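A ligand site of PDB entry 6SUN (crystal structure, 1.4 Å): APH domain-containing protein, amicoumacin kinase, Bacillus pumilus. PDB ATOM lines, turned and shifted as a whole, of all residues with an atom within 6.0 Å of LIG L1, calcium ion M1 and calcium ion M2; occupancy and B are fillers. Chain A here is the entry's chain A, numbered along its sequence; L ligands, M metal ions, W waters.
A nitrogen (N5) of LIG L1 lies within hydrogen-bond range of the backbone NH (N) of Ala 113 (2.9 Å).
NZ of Lys 53 is in salt-bridge range of O6 of LIG L1 (2.7 Å).
The side-chain amino group (NZ) of Lys 117 sits at hydrogen-bond distance from an oxygen (O11) of LIG L1, at 2.8 Å.
A nitrogen (N4) of LIG L1 lies within hydrogen-bond range of the backbone carbonyl oxygen (O) of Glu 111 (3.2 Å).
The side-chain carboxylate of Asp 223 is in salt-bridge range of a nitrogen (N2) of LG2 L2, at 2.8 Å.
The backbone NH (N) of Gly 207 sits close to an oxygen (O1) of LG2 L2.
The backbone NH (N) of Asn 37 is in hydrogen-bond range of an oxygen (O4) of LIG L1 (3.3 Å).
The side-chain carboxylate (OD2) of Asp 203 lies within salt-bridge range of a nitrogen (N2) of LG2 L2 (3.9 Å).
ND2 of Asn 37 is in hydrogen-bond range of O4 of LIG L1 (3.1 Å).
N of Ala 83 sits at hydrogen-bond distance from O of Ala 218 (3.1 Å).
The backbone carbonyl oxygen of Val 39 sits at hydrogen-bond distance from the backbone NH of Leu 32 (2.8 Å).
The backbone carbonyl oxygen (O) of Ala 113 is in hydrogen-bond range of a ring nitrogen (ND1) of His 210 (3.1 Å).
The backbone NH (N) of Ile 51 is in hydrogen-bond range of the backbone carbonyl oxygen (O) of Tyr 110, 2.9 Å away.
NZ of Lys 53 lies close to OD2 of Asp 222, at 3.1 Å.
The backbone NH of Gly 207 is in hydrogen-bond range of a ring nitrogen (ND1) of His 205, 2.9 Å away.
OD1 of Asp 220 sits close to NZ of Lys 53, 3.1 Å away.
O of Asn 208 lies within hydrogen-bond range of N of Phe 219.
CD1 of Leu 32 touches O10 of LIG L1 (3.7 Å).
CB of Glu 36 touches O4 of LIG L1, at 3.6 Å.
Val 39 touches LIG L1.
CG1 of Ile 51 touches C7 of LIG L1, at 3.6 Å.
Ala 83 touches LIG L1 (CB to N4, 3.2 Å).
CA of Lys 112 touches N5 of LIG L1 (3.5 Å).
Gly 207 touches LIG L1.
His 210 touches LIG L1.
Phe 219 touches LIG L1.
Hydrophobic or aromatic side chains within 4 Å of LIG L1: Leu 32, Val 39, Ile 51, Ala 83, Ala 113, His 210 and Phe 219.
Of the 25 residues printed, 17 come within 4 Å of LIG L1.
Of the 25 residues printed, 2 come within 4 Å of calcium ion M1.
Along chain A the residues within 4 Å of calcium ion M1 span positions 208 to 220.
Calcium ion M1 is bound by the side-chain carboxylate (OD2) of Asp 220 (2.3 Å), an oxygen (O7) of LIG L1 (2.3 Å), water W9 (2.4 Å), the side-chain amide oxygen (OD1) of Asn 208 (2.4 Å), an oxygen (O3) of LIG L1 (2.4 Å), water W12 (2.4 Å) and an oxygen (O1) of LIG L1 (2.6 Å).
Calcium ion M2 is bound by O1 of LIG L1, 2.3 Å away.
Water W14 is bound to calcium ion M2, 2.3 Å away.
An oxygen (O5) of LIG L1 is bound to calcium ion M2.
Water W16 binds calcium ion M2 (2.4 Å).
Calcium ion M2 is bound by the side-chain carboxylate (OD1) of Asp 220 (2.5 Å).
OD2 of Asp 220 binds calcium ion M2.
The side-chain carboxylate (OD2) of Asp 222 is bound to calcium ion M2.
OD1 of Asp 222 binds calcium ion M2 (2.7 Å).
Calcium ion M2 has eight donor atoms within binding distance.
Water W12 lies within hydrogen-bond range of the side-chain carboxylate (OD2) of Asp 203 (2.8 Å), a ring nitrogen (NE2) of His 205 (2.9 Å), the side-chain amide nitrogen (ND2) of Asn 208 (3.2 Å) and an oxygen (O5) of LG2 L2 (3.4 Å).
Water W16 bridges OD2 of Asp 223 (2.6 Å) and OD2 of Asp 203 (2.7 Å).
Water W2 bridges an oxygen (O12) of LIG L1 (2.8 Å) and a ring nitrogen (NE2) of His 210 (2.8 Å).
Water W8 lies within hydrogen-bond range of O6 of LIG L1 (2.8 Å) and N of Asp 220 (3.0 Å).
Water W3 bridges O2 of LIG L1 (2.9 Å) and N1 of LG2 L2 (3.0 Å).
Water W1 lies within hydrogen-bond range of OE2 of Glu 36 (2.7 Å), O2 of LIG L1 (2.9 Å) and N2 of LG2 L2 (3.2 Å).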
ATOM      1  N   LEU A  32       5.606  12.667  -4.190  1.00  0.00           N
ATOM      2  CA  LEU A  32       4.877  11.962  -5.259  1.00  0.00           C
ATOM      3  C   LEU A  32       5.611  10.769  -5.848  1.00  0.00           C
ATOM      4  O   LEU A  32       4.980   9.759  -6.089  1.00  0.00           O
ATOM      5  CB  LEU A  32       4.524  12.913  -6.412  1.00  0.00           C
ATOM      6  CG  LEU A  32       3.694  14.149  -6.066  1.00  0.00           C
ATOM      7  CD1 LEU A  32       3.389  14.935  -7.321  1.00  0.00           C
ATOM      8  CD2 LEU A  32       2.399  13.750  -5.358  1.00  0.00           C
ATOM      9  N   ALA A  33       6.912  10.920  -6.126  1.00  0.00           N
ATOM     10  CA  ALA A  33       7.658   9.872  -6.815  1.00  0.00           C
ATOM     11  C   ALA A  33       9.161   9.997  -6.611  1.00  0.00           C
ATOM     12  O   ALA A  33       9.666  11.098  -6.358  1.00  0.00           O
ATOM     13  CB  ALA A  33       7.356   9.911  -8.295  1.00  0.00           C
ATOM     14  N   ALA A  35      11.274   7.258  -8.481  1.00  0.00           N
ATOM     15  CA  ALA A  35      11.843   6.172  -9.280  1.00  0.00           C
ATOM     16  C   ALA A  35      12.846   6.705 -10.288  1.00  0.00           C
ATOM     17  O   ALA A  35      13.864   6.058 -10.521  1.00  0.00           O
ATOM     18  CB  ALA A  35      10.741   5.370  -9.981  1.00  0.00           C
ATOM     19  N   GLU A  36      12.556   7.857 -10.891  1.00  0.00           N
ATOM     20  CA  GLU A  36      13.350   8.452 -11.969  1.00  0.00           C
ATOM     21  C   GLU A  36      13.995   9.788 -11.531  1.00  0.00           C
ATOM     22  O   GLU A  36      15.199   9.994 -11.618  1.00  0.00           O
ATOM     23  CB  GLU A  36      12.426   8.648 -13.180  1.00  0.00           C
ATOM     24  CG  GLU A  36      13.117   8.731 -14.522  1.00  0.00           C
ATOM     25  CD  GLU A  36      13.411   7.359 -15.108  1.00  0.00           C
ATOM     26  OE1 GLU A  36      14.330   6.691 -14.596  1.00  0.00           O
ATOM     27  OE2 GLU A  36      12.721   6.952 -16.078  1.00  0.00           O
ATOM     28  N   ASN A  37      13.147  10.699 -11.087  1.00  0.00           N
ATOM     29  CA  ASN A  37      13.497  11.982 -10.483  1.00  0.00           C
ATOM     30  C   ASN A  37      12.842  11.975  -9.116  1.00  0.00           C
ATOM     31  O   ASN A  37      11.959  11.151  -8.856  1.00  0.00           O
ATOM     32  CB  ASN A  37      12.891  13.117 -11.303  1.00  0.00           C
ATOM     33  CG  ASN A  37      13.400  13.149 -12.713  1.00  0.00           C
ATOM     34  OD1 ASN A  37      14.498  13.595 -12.963  1.00  0.00           O
ATOM     35  ND2 ASN A  37      12.580  12.698 -13.650  1.00  0.00           N
ATOM     36  N   TYR A  38      13.218  12.921  -8.241  1.00  0.00           N
ATOM     37  CA  TYR A  38      12.421  13.151  -7.029  1.00  0.00           C
ATOM     38  C   TYR A  38      11.346  14.168  -7.377  1.00  0.00           C
ATOM     39  O   TYR A  38      11.665  15.240  -7.855  1.00  0.00           O
ATOM     40  CB  TYR A  38      13.255  13.666  -5.872  1.00  0.00           C
ATOM     41  CG  TYR A  38      14.340  12.753  -5.401  1.00  0.00           C
ATOM     42  CD1 TYR A  38      14.044  11.617  -4.666  1.00  0.00           C
ATOM     43  CD2 TYR A  38      15.669  13.039  -5.672  1.00  0.00           C
ATOM     44  CE1 TYR A  38      15.070  10.777  -4.205  1.00  0.00           C
ATOM     45  CE2 TYR A  38      16.687  12.210  -5.216  1.00  0.00           C
ATOM     46  CZ  TYR A  38      16.381  11.081  -4.514  1.00  0.00           C
ATOM     47  OH  TYR A  38      17.428  10.283  -4.069  1.00  0.00           O
ATOM     48  N   VAL A  39      10.088  13.818  -7.139  1.00  0.00           N
ATOM     49  CA  VAL A  39       8.966  14.672  -7.519  1.00  0.00           C
ATOM     50  C   VAL A  39       8.096  14.898  -6.291  1.00  0.00           C
ATOM     51  O   VAL A  39       7.708  13.942  -5.571  1.00  0.00           O
ATOM     52  CB  VAL A  39       8.115  14.075  -8.678  1.00  0.00           C
ATOM     53  CG1 VAL A  39       7.085  15.084  -9.171  1.00  0.00           C
ATOM     54  CG2 VAL A  39       9.008  13.644  -9.838  1.00  0.00           C
ATOM     55  N   ILE A  51       4.479  21.718  -8.843  1.00  0.00           N
ATOM     56  CA  ILE A  51       5.211  20.472  -8.884  1.00  0.00           C
ATOM     57  C   ILE A  51       6.703  20.800  -8.916  1.00  0.00           C
ATOM     58  O   ILE A  51       7.162  21.530  -9.797  1.00  0.00           O
ATOM     59  CB  ILE A  51       4.812  19.613 -10.102  1.00  0.00           C
ATOM     60  CG1 ILE A  51       3.311  19.248 -10.036  1.00  0.00           C
ATOM     61  CG2 ILE A  51       5.718  18.388 -10.241  1.00  0.00           C
ATOM     62  CD1 ILE A  51       2.913  18.251  -8.966  1.00  0.00           C
ATOM     63  N   LYS A  53      10.414  19.124  -9.298  1.00  0.00           N
ATOM     64  CA  LYS A  53      11.117  17.949  -9.811  1.00  0.00           C
ATOM     65  C   LYS A  53      12.599  18.188  -9.594  1.00  0.00           C
ATOM     66  O   LYS A  53      13.136  19.269  -9.919  1.00  0.00           O
ATOM     67  CB  LYS A  53      10.828  17.753 -11.311  1.00  0.00           C
ATOM     68  CG  LYS A  53      11.609  16.605 -11.950  1.00  0.00           C
ATOM     69  CD  LYS A  53      11.202  16.354 -13.401  1.00  0.00           C
ATOM     70  CE  LYS A  53      10.127  15.307 -13.488  1.00  0.00           C
ATOM     71  NZ  LYS A  53       9.697  14.942 -14.878  1.00  0.00           N
ATOM     72  N   ALA A  83       1.880  22.523 -18.753  1.00  0.00           N
ATOM     73  CA  ALA A  83       2.255  22.899 -17.384  1.00  0.00           C
ATOM     74  C   ALA A  83       3.499  23.772 -17.461  1.00  0.00           C
ATOM     75  O   ALA A  83       4.575  23.299 -17.768  1.00  0.00           O
ATOM     76  CB  ALA A  83       2.521  21.664 -16.542  1.00  0.00           C
ATOM     77  N   TYR A 110       7.115  23.498 -11.909  1.00  0.00           N
ATOM     78  CA  TYR A 110       6.067  23.773 -12.886  1.00  0.00           C
ATOM     79  C   TYR A 110       4.768  24.026 -12.157  1.00  0.00           C
ATOM     80  O   TYR A 110       4.529  23.533 -11.056  1.00  0.00           O
ATOM     81  CB  TYR A 110       5.861  22.553 -13.775  1.00  0.00           C
ATOM     82  CG  TYR A 110       7.106  21.973 -14.398  1.00  0.00           C
ATOM     83  CD1 TYR A 110       7.487  22.303 -15.682  1.00  0.00           C
ATOM     84  CD2 TYR A 110       7.874  21.050 -13.704  1.00  0.00           C
ATOM     85  CE1 TYR A 110       8.619  21.732 -16.255  1.00  0.00           C
ATOM     86  CE2 TYR A 110       8.984  20.459 -14.268  1.00  0.00           C
ATOM     87  CZ  TYR A 110       9.356  20.800 -15.532  1.00  0.00           C
ATOM     88  OH  TYR A 110      10.457  20.179 -16.070  1.00  0.00           O
ATOM     89  N   GLU A 111       3.878  24.751 -12.827  1.00  0.00           N
ATOM     90  CA  GLU A 111       2.498  24.824 -12.376  1.00  0.00           C
ATOM     91  C   GLU A 111       1.871  23.425 -12.376  1.00  0.00           C
ATOM     92  O   GLU A 111       2.111  22.634 -13.285  1.00  0.00           O
ATOM     93  CB  GLU A 111       1.683  25.762 -13.281  1.00  0.00           C
ATOM     94  CG  GLU A 111       2.165  27.204 -13.155  1.00  0.00           C
ATOM     95  CD  GLU A 111       1.373  28.240 -13.928  1.00  0.00           C
ATOM     96  OE1 GLU A 111       0.340  27.900 -14.536  1.00  0.00           O
ATOM     97  OE2 GLU A 111       1.806  29.415 -13.942  1.00  0.00           O
ATOM     98  N   LYS A 112       1.049  23.121 -11.363  1.00  0.00           N
ATOM     99  CA  LYS A 112       0.288  21.855 -11.370  1.00  0.00           C
ATOM    100  C   LYS A 112      -0.827  21.995 -12.383  1.00  0.00           C
ATOM    101  O   LYS A 112      -1.683  22.857 -12.223  1.00  0.00           O
ATOM    102  CB  LYS A 112      -0.283  21.538  -9.987  1.00  0.00           C
ATOM    103  CG  LYS A 112      -0.956  20.173  -9.912  1.00  0.00           C
ATOM    104  CD  LYS A 112      -1.648  19.957  -8.574  1.00  0.00           C
ATOM    105  CE  LYS A 112      -2.221  18.569  -8.497  1.00  0.00           C
ATOM    106  NZ  LYS A 112      -2.931  18.388  -7.197  1.00  0.00           N
ATOM    107  N   ALA A 113      -0.852  21.120 -13.380  1.00  0.00           N
ATOM    108  CA  ALA A 113      -1.912  21.124 -14.383  1.00  0.00           C
ATOM    109  C   ALA A 113      -3.262  20.921 -13.714  1.00  0.00           C
ATOM    110  O   ALA A 113      -3.388  20.081 -12.844  1.00  0.00           O
ATOM    111  CB  ALA A 113      -1.674  20.021 -15.400  1.00  0.00           C
ATOM    112  N   LYS A 117      -5.838  12.851 -14.261  1.00  0.00           N
ATOM    113  CA  LYS A 117      -5.643  11.893 -15.333  1.00  0.00           C
ATOM    114  C   LYS A 117      -6.957  11.301 -15.819  1.00  0.00           C
ATOM    115  O   LYS A 117      -7.938  11.221 -15.061  1.00  0.00           O
ATOM    116  CB  LYS A 117      -4.639  10.804 -14.893  1.00  0.00           C
ATOM    117  CG  LYS A 117      -3.222  11.376 -14.685  1.00  0.00           C
ATOM    118  CD  LYS A 117      -2.263  10.348 -14.123  1.00  0.00           C
ATOM    119  CE  LYS A 117      -0.911  10.977 -13.861  1.00  0.00           C
ATOM    120  NZ  LYS A 117       0.013  10.012 -13.213  1.00  0.00           N
ATOM    121  N   ASP A 203       7.111  11.385 -25.157  1.00  0.00           N
ATOM    122  CA  ASP A 203       6.648  10.455 -24.103  1.00  0.00           C
ATOM    123  C   ASP A 203       5.161  10.718 -23.854  1.00  0.00           C
ATOM    124  O   ASP A 203       4.717  10.819 -22.693  1.00  0.00           O
ATOM    125  CB  ASP A 203       7.474  10.655 -22.813  1.00  0.00           C
ATOM    126  CG  ASP A 203       7.247   9.557 -21.759  1.00  0.00           C
ATOM    127  OD1 ASP A 203       6.863   8.451 -22.134  1.00  0.00           O
ATOM    128  OD2 ASP A 203       7.488   9.842 -20.551  1.00  0.00           O
ATOM    129  N   HIS A 205       1.464   9.924 -23.290  1.00  0.00           N
ATOM    130  CA  HIS A 205       0.578   8.897 -22.795  1.00  0.00           C
ATOM    131  C   HIS A 205      -0.240   9.514 -21.686  1.00  0.00           C
ATOM    132  O   HIS A 205       0.040  10.609 -21.212  1.00  0.00           O
ATOM    133  CB  HIS A 205       1.321   7.642 -22.316  1.00  0.00           C
ATOM    134  CG  HIS A 205       2.304   7.867 -21.226  1.00  0.00           C
ATOM    135  ND1 HIS A 205       1.949   8.209 -19.941  1.00  0.00           N
ATOM    136  CD2 HIS A 205       3.655   7.846 -21.253  1.00  0.00           C
ATOM    137  CE1 HIS A 205       3.041   8.337 -19.203  1.00  0.00           C
ATOM    138  NE2 HIS A 205       4.094   8.131 -19.978  1.00  0.00           N
ATOM    139  N   GLY A 207      -0.530   8.866 -18.584  1.00  0.00           N
ATOM    140  CA  GLY A 207       0.138   9.235 -17.352  1.00  0.00           C
ATOM    141  C   GLY A 207       0.846  10.580 -17.350  1.00  0.00           C
ATOM    142  O   GLY A 207       1.327  11.007 -16.304  1.00  0.00           O
ATOM    143  N   ASN A 208       0.899  11.240 -18.511  1.00  0.00           N
ATOM    144  CA  ASN A 208       1.684  12.460 -18.693  1.00  0.00           C
ATOM    145  C   ASN A 208       0.841  13.668 -19.153  1.00  0.00           C
ATOM    146  O   ASN A 208       1.371  14.653 -19.633  1.00  0.00           O
ATOM    147  CB  ASN A 208       2.824  12.258 -19.676  1.00  0.00           C
ATOM    148  CG  ASN A 208       4.037  11.611 -19.060  1.00  0.00           C
ATOM    149  OD1 ASN A 208       4.200  11.514 -17.829  1.00  0.00           O
ATOM    150  ND2 ASN A 208       4.985  11.295 -19.931  1.00  0.00           N
ATOM    151  N   HIS A 210      -3.108  15.865 -18.026  1.00  0.00           N
ATOM    152  CA  HIS A 210      -4.403  15.932 -17.381  1.00  0.00           C
ATOM    153  C   HIS A 210      -5.467  16.318 -18.387  1.00  0.00           C
ATOM    154  O   HIS A 210      -5.184  16.919 -19.410  1.00  0.00           O
ATOM    155  CB  HIS A 210      -4.396  16.943 -16.226  1.00  0.00           C
ATOM    156  CG  HIS A 210      -3.746  16.430 -14.982  1.00  0.00           C
ATOM    157  ND1 HIS A 210      -3.611  17.211 -13.860  1.00  0.00           N
ATOM    158  CD2 HIS A 210      -3.184  15.239 -14.685  1.00  0.00           C
ATOM    159  CE1 HIS A 210      -3.010  16.504 -12.916  1.00  0.00           C
ATOM    160  NE2 HIS A 210      -2.737  15.309 -13.388  1.00  0.00           N
ATOM    161  N   ALA A 218      -0.526  18.832 -21.032  1.00  0.00           N
ATOM    162  CA  ALA A 218       0.597  17.916 -20.894  1.00  0.00           C
ATOM    163  C   ALA A 218       1.661  18.430 -19.939  1.00  0.00           C
ATOM    164  O   ALA A 218       1.862  19.640 -19.751  1.00  0.00           O
ATOM    165  CB  ALA A 218       1.222  17.620 -22.249  1.00  0.00           C
ATOM    166  N   PHE A 219       2.389  17.465 -19.383  1.00  0.00           N
ATOM    167  CA  PHE A 219       3.542  17.700 -18.528  1.00  0.00           C
ATOM    168  C   PHE A 219       4.565  16.592 -18.808  1.00  0.00           C
ATOM    169  O   PHE A 219       4.441  15.827 -19.788  1.00  0.00           O
ATOM    170  CB  PHE A 219       3.125  17.814 -17.046  1.00  0.00           C
ATOM    171  CG  PHE A 219       2.236  16.712 -16.560  1.00  0.00           C
ATOM    172  CD1 PHE A 219       2.766  15.509 -16.172  1.00  0.00           C
ATOM    173  CD2 PHE A 219       0.878  16.892 -16.471  1.00  0.00           C
ATOM    174  CE1 PHE A 219       1.958  14.489 -15.742  1.00  0.00           C
ATOM    175  CE2 PHE A 219       0.038  15.881 -16.011  1.00  0.00           C
ATOM    176  CZ  PHE A 219       0.592  14.668 -15.641  1.00  0.00           C
ATOM    177  N   ASP A 220       5.620  16.551 -17.989  1.00  0.00           N
ATOM    178  CA  ASP A 220       6.701  15.579 -18.143  1.00  0.00           C
ATOM    179  C   ASP A 220       7.331  15.569 -19.538  1.00  0.00           C
ATOM    180  O   ASP A 220       7.299  14.597 -20.240  1.00  0.00           O
ATOM    181  CB  ASP A 220       6.241  14.173 -17.738  1.00  0.00           C
ATOM    182  CG  ASP A 220       7.420  13.206 -17.572  1.00  0.00           C
ATOM    183  OD1 ASP A 220       8.582  13.692 -17.516  1.00  0.00           O
ATOM    184  OD2 ASP A 220       7.210  11.967 -17.540  1.00  0.00           O
ATOM    185  N   ASP A 222      10.419  15.653 -19.973  1.00  0.00           N
ATOM    186  CA  ASP A 222      11.818  15.384 -19.759  1.00  0.00           C
ATOM    187  C   ASP A 222      12.525  14.494 -20.851  1.00  0.00           C
ATOM    188  O   ASP A 222      13.749  14.500 -20.969  1.00  0.00           O
ATOM    189  CB  ASP A 222      12.052  15.000 -18.290  1.00  0.00           C
ATOM    190  CG  ASP A 222      11.570  13.632 -17.959  1.00  0.00           C
ATOM    191  OD1 ASP A 222      11.218  12.863 -18.870  1.00  0.00           O
ATOM    192  OD2 ASP A 222      11.503  13.298 -16.743  1.00  0.00           O
ATOM    193  N   ASP A 223      11.749  13.822 -21.705  1.00  0.00           N
ATOM    194  CA  ASP A 223      12.350  13.089 -22.808  1.00  0.00           C
ATOM    195  C   ASP A 223      12.223  13.802 -24.159  1.00  0.00           C
ATOM    196  O   ASP A 223      12.532  13.219 -25.192  1.00  0.00           O
ATOM    197  CB  ASP A 223      11.791  11.678 -22.838  1.00  0.00           C
ATOM    198  CG  ASP A 223      12.286  10.849 -21.667  1.00  0.00           C
ATOM    199  OD1 ASP A 223      13.517  10.835 -21.403  1.00  0.00           O
ATOM    200  OD2 ASP A 223      11.447  10.214 -20.996  1.00  0.00           O
HETATM  201  P1  LIG L   1       8.137   8.936 -15.042  1.00  0.00           P
HETATM  202  O1  LIG L   1       8.353   9.831 -16.221  1.00  0.00           O
HETATM  203  O2  LIG L   1       8.802   7.595 -15.088  1.00  0.00           O
HETATM  204  O3  LIG L   1       6.618   8.881 -14.820  1.00  0.00           O
HETATM  205  P2  LIG L   1       9.206  11.300 -13.492  1.00  0.00           P
HETATM  206  O4  LIG L   1      10.161  11.364 -12.340  1.00  0.00           O
HETATM  207  O5  LIG L   1       9.661  11.901 -14.784  1.00  0.00           O
HETATM  208  N1  LIG L   1       8.739   9.674 -13.623  1.00  0.00           N
HETATM  209  P3  LIG L   1       6.717  12.851 -13.717  1.00  0.00           P
HETATM  210  O6  LIG L   1       7.211  14.143 -14.248  1.00  0.00           O
HETATM  211  O7  LIG L   1       5.945  11.936 -14.573  1.00  0.00           O
HETATM  212  O8  LIG L   1       7.891  12.090 -12.963  1.00  0.00           O
HETATM  213  O9  LIG L   1       5.863  13.196 -12.430  1.00  0.00           O
HETATM  214  C1  LIG L   1       5.313  12.179 -11.580  1.00  0.00           C
HETATM  215  C2  LIG L   1       3.835  12.444 -11.343  1.00  0.00           C
HETATM  216  O10 LIG L   1       3.624  13.734 -10.764  1.00  0.00           O
HETATM  217  C3  LIG L   1       2.962  12.401 -12.600  1.00  0.00           C
HETATM  218  O11 LIG L   1       2.621  11.080 -13.015  1.00  0.00           O
HETATM  219  C4  LIG L   1       1.779  13.239 -12.189  1.00  0.00           C
HETATM  220  O12 LIG L   1       0.869  12.473 -11.398  1.00  0.00           O
HETATM  221  C5  LIG L   1       2.442  14.301 -11.365  1.00  0.00           C
HETATM  222  N2  LIG L   1       2.880  15.492 -12.123  1.00  0.00           N
HETATM  223  C6  LIG L   1       4.111  15.769 -12.652  1.00  0.00           C
HETATM  224  N3  LIG L   1       4.144  16.959 -13.225  1.00  0.00           N
HETATM  225  C7  LIG L   1       2.905  17.456 -13.116  1.00  0.00           C
HETATM  226  C8  LIG L   1       2.286  18.715 -13.441  1.00  0.00           C
HETATM  227  N4  LIG L   1       2.961  19.662 -14.055  1.00  0.00           N
HETATM  228  N5  LIG L   1       0.985  18.888 -13.161  1.00  0.00           N
HETATM  229  C9  LIG L   1       0.270  17.937 -12.515  1.00  0.00           C
HETATM  230  N6  LIG L   1       0.783  16.773 -12.110  1.00  0.00           N
HETATM  231  C10 LIG L   1       2.069  16.490 -12.402  1.00  0.00           C
HETATM  232  C1  LG2 L   2       4.104   3.969 -20.085  1.00  0.00           C
HETATM  233  C2  LG2 L   2       2.654   4.317 -19.881  1.00  0.00           C
HETATM  234  C3  LG2 L   2       1.750   4.023 -20.892  1.00  0.00           C
HETATM  235  C4  LG2 L   2       0.402   4.360 -20.702  1.00  0.00           C
HETATM  236  C5  LG2 L   2       0.019   4.997 -19.543  1.00  0.00           C
HETATM  237  C6  LG2 L   2       0.916   5.273 -18.521  1.00  0.00           C
HETATM  238  O1  LG2 L   2       0.536   5.882 -17.372  1.00  0.00           O
HETATM  239  C7  LG2 L   2       2.258   4.930 -18.716  1.00  0.00           C
HETATM  240  C8  LG2 L   2       3.270   5.245 -17.667  1.00  0.00           C
HETATM  241  O2  LG2 L   2       3.059   6.014 -16.749  1.00  0.00           O
HETATM  242  O3  LG2 L   2       4.579   4.754 -17.829  1.00  0.00           O
HETATM  243  C9  LG2 L   2       4.746   3.652 -18.723  1.00  0.00           C
HETATM  244  C10 LG2 L   2       6.217   3.357 -18.818  1.00  0.00           C
HETATM  245  C11 LG2 L   2       6.766   2.982 -17.433  1.00  0.00           C
HETATM  246  C12 LG2 L   2       8.225   2.572 -17.442  1.00  0.00           C
HETATM  247  C13 LG2 L   2       8.661   2.350 -15.995  1.00  0.00           C
HETATM  248  C14 LG2 L   2       8.485   1.351 -18.295  1.00  0.00           C
HETATM  249  N1  LG2 L   2       6.946   4.512 -19.364  1.00  0.00           N
HETATM  250  C15 LG2 L   2       7.464   4.498 -20.579  1.00  0.00           C
HETATM  251  O4  LG2 L   2       7.399   3.515 -21.306  1.00  0.00           O
HETATM  252  C16 LG2 L   2       8.170   5.749 -21.089  1.00  0.00           C
HETATM  253  O5  LG2 L   2       8.054   6.830 -20.195  1.00  0.00           O
HETATM  254  C17 LG2 L   2       9.669   5.461 -21.304  1.00  0.00           C
HETATM  255  O6  LG2 L   2       9.767   4.508 -22.341  1.00  0.00           O
HETATM  256  C18 LG2 L   2      10.441   6.694 -21.759  1.00  0.00           C
HETATM  257  N2  LG2 L   2      10.691   7.579 -20.622  1.00  0.00           N
HETATM  258  C19 LG2 L   2      11.761   6.294 -22.425  1.00  0.00           C
HETATM  259  C20 LG2 L   2      12.533   7.457 -22.974  1.00  0.00           C
HETATM  260  O7  LG2 L   2      11.996   8.343 -23.616  1.00  0.00           O
HETATM  261  N3  LG2 L   2      13.815   7.466 -22.661  1.00  0.00           N
HETATM  262 CA    CA M   1       5.855  10.528 -16.398  1.00  0.00          CA
HETATM  263 CA    CA M   2       9.636  11.506 -17.078  1.00  0.00          CA
HETATM  264  O   HOH W   1      10.444   7.429 -17.477  1.00  0.00           O
HETATM  265  O   HOH W   2      -1.650  13.567 -11.553  1.00  0.00           O
HETATM  266  O   HOH W   3       7.182   6.510 -17.184  1.00  0.00           O
HETATM  267  O   HOH W   4       5.708  19.301 -15.373  1.00  0.00           O
HETATM  268  O   HOH W   5       1.095  11.495  -8.878  1.00  0.00           O
HETATM  269  O   HOH W   6      -0.812  15.744 -10.094  1.00  0.00           O
HETATM  270  O   HOH W   7       9.016   5.833 -13.081  1.00  0.00           O
HETATM  271  O   HOH W   8       6.278  16.627 -15.055  1.00  0.00           O
HETATM  272  O   HOH W   9       3.726   9.804 -15.629  1.00  0.00           O
HETATM  273  O   HOH W  10       8.338   7.787 -11.174  1.00  0.00           O
HETATM  274  O   HOH W  11       5.641   8.869 -12.379  1.00  0.00           O
HETATM  275  O   HOH W  12       6.290   8.920 -18.188  1.00  0.00           O
HETATM  276  O   HOH W  13      10.286   9.620 -10.556  1.00  0.00           O
HETATM  277  O   HOH W  14      11.413  10.092 -17.287  1.00  0.00           O
HETATM  278  O   HOH W  15       5.420   6.325 -14.968  1.00  0.00           O
HETATM  279  O   HOH W  16       9.548  11.162 -19.412  1.00  0.00           O
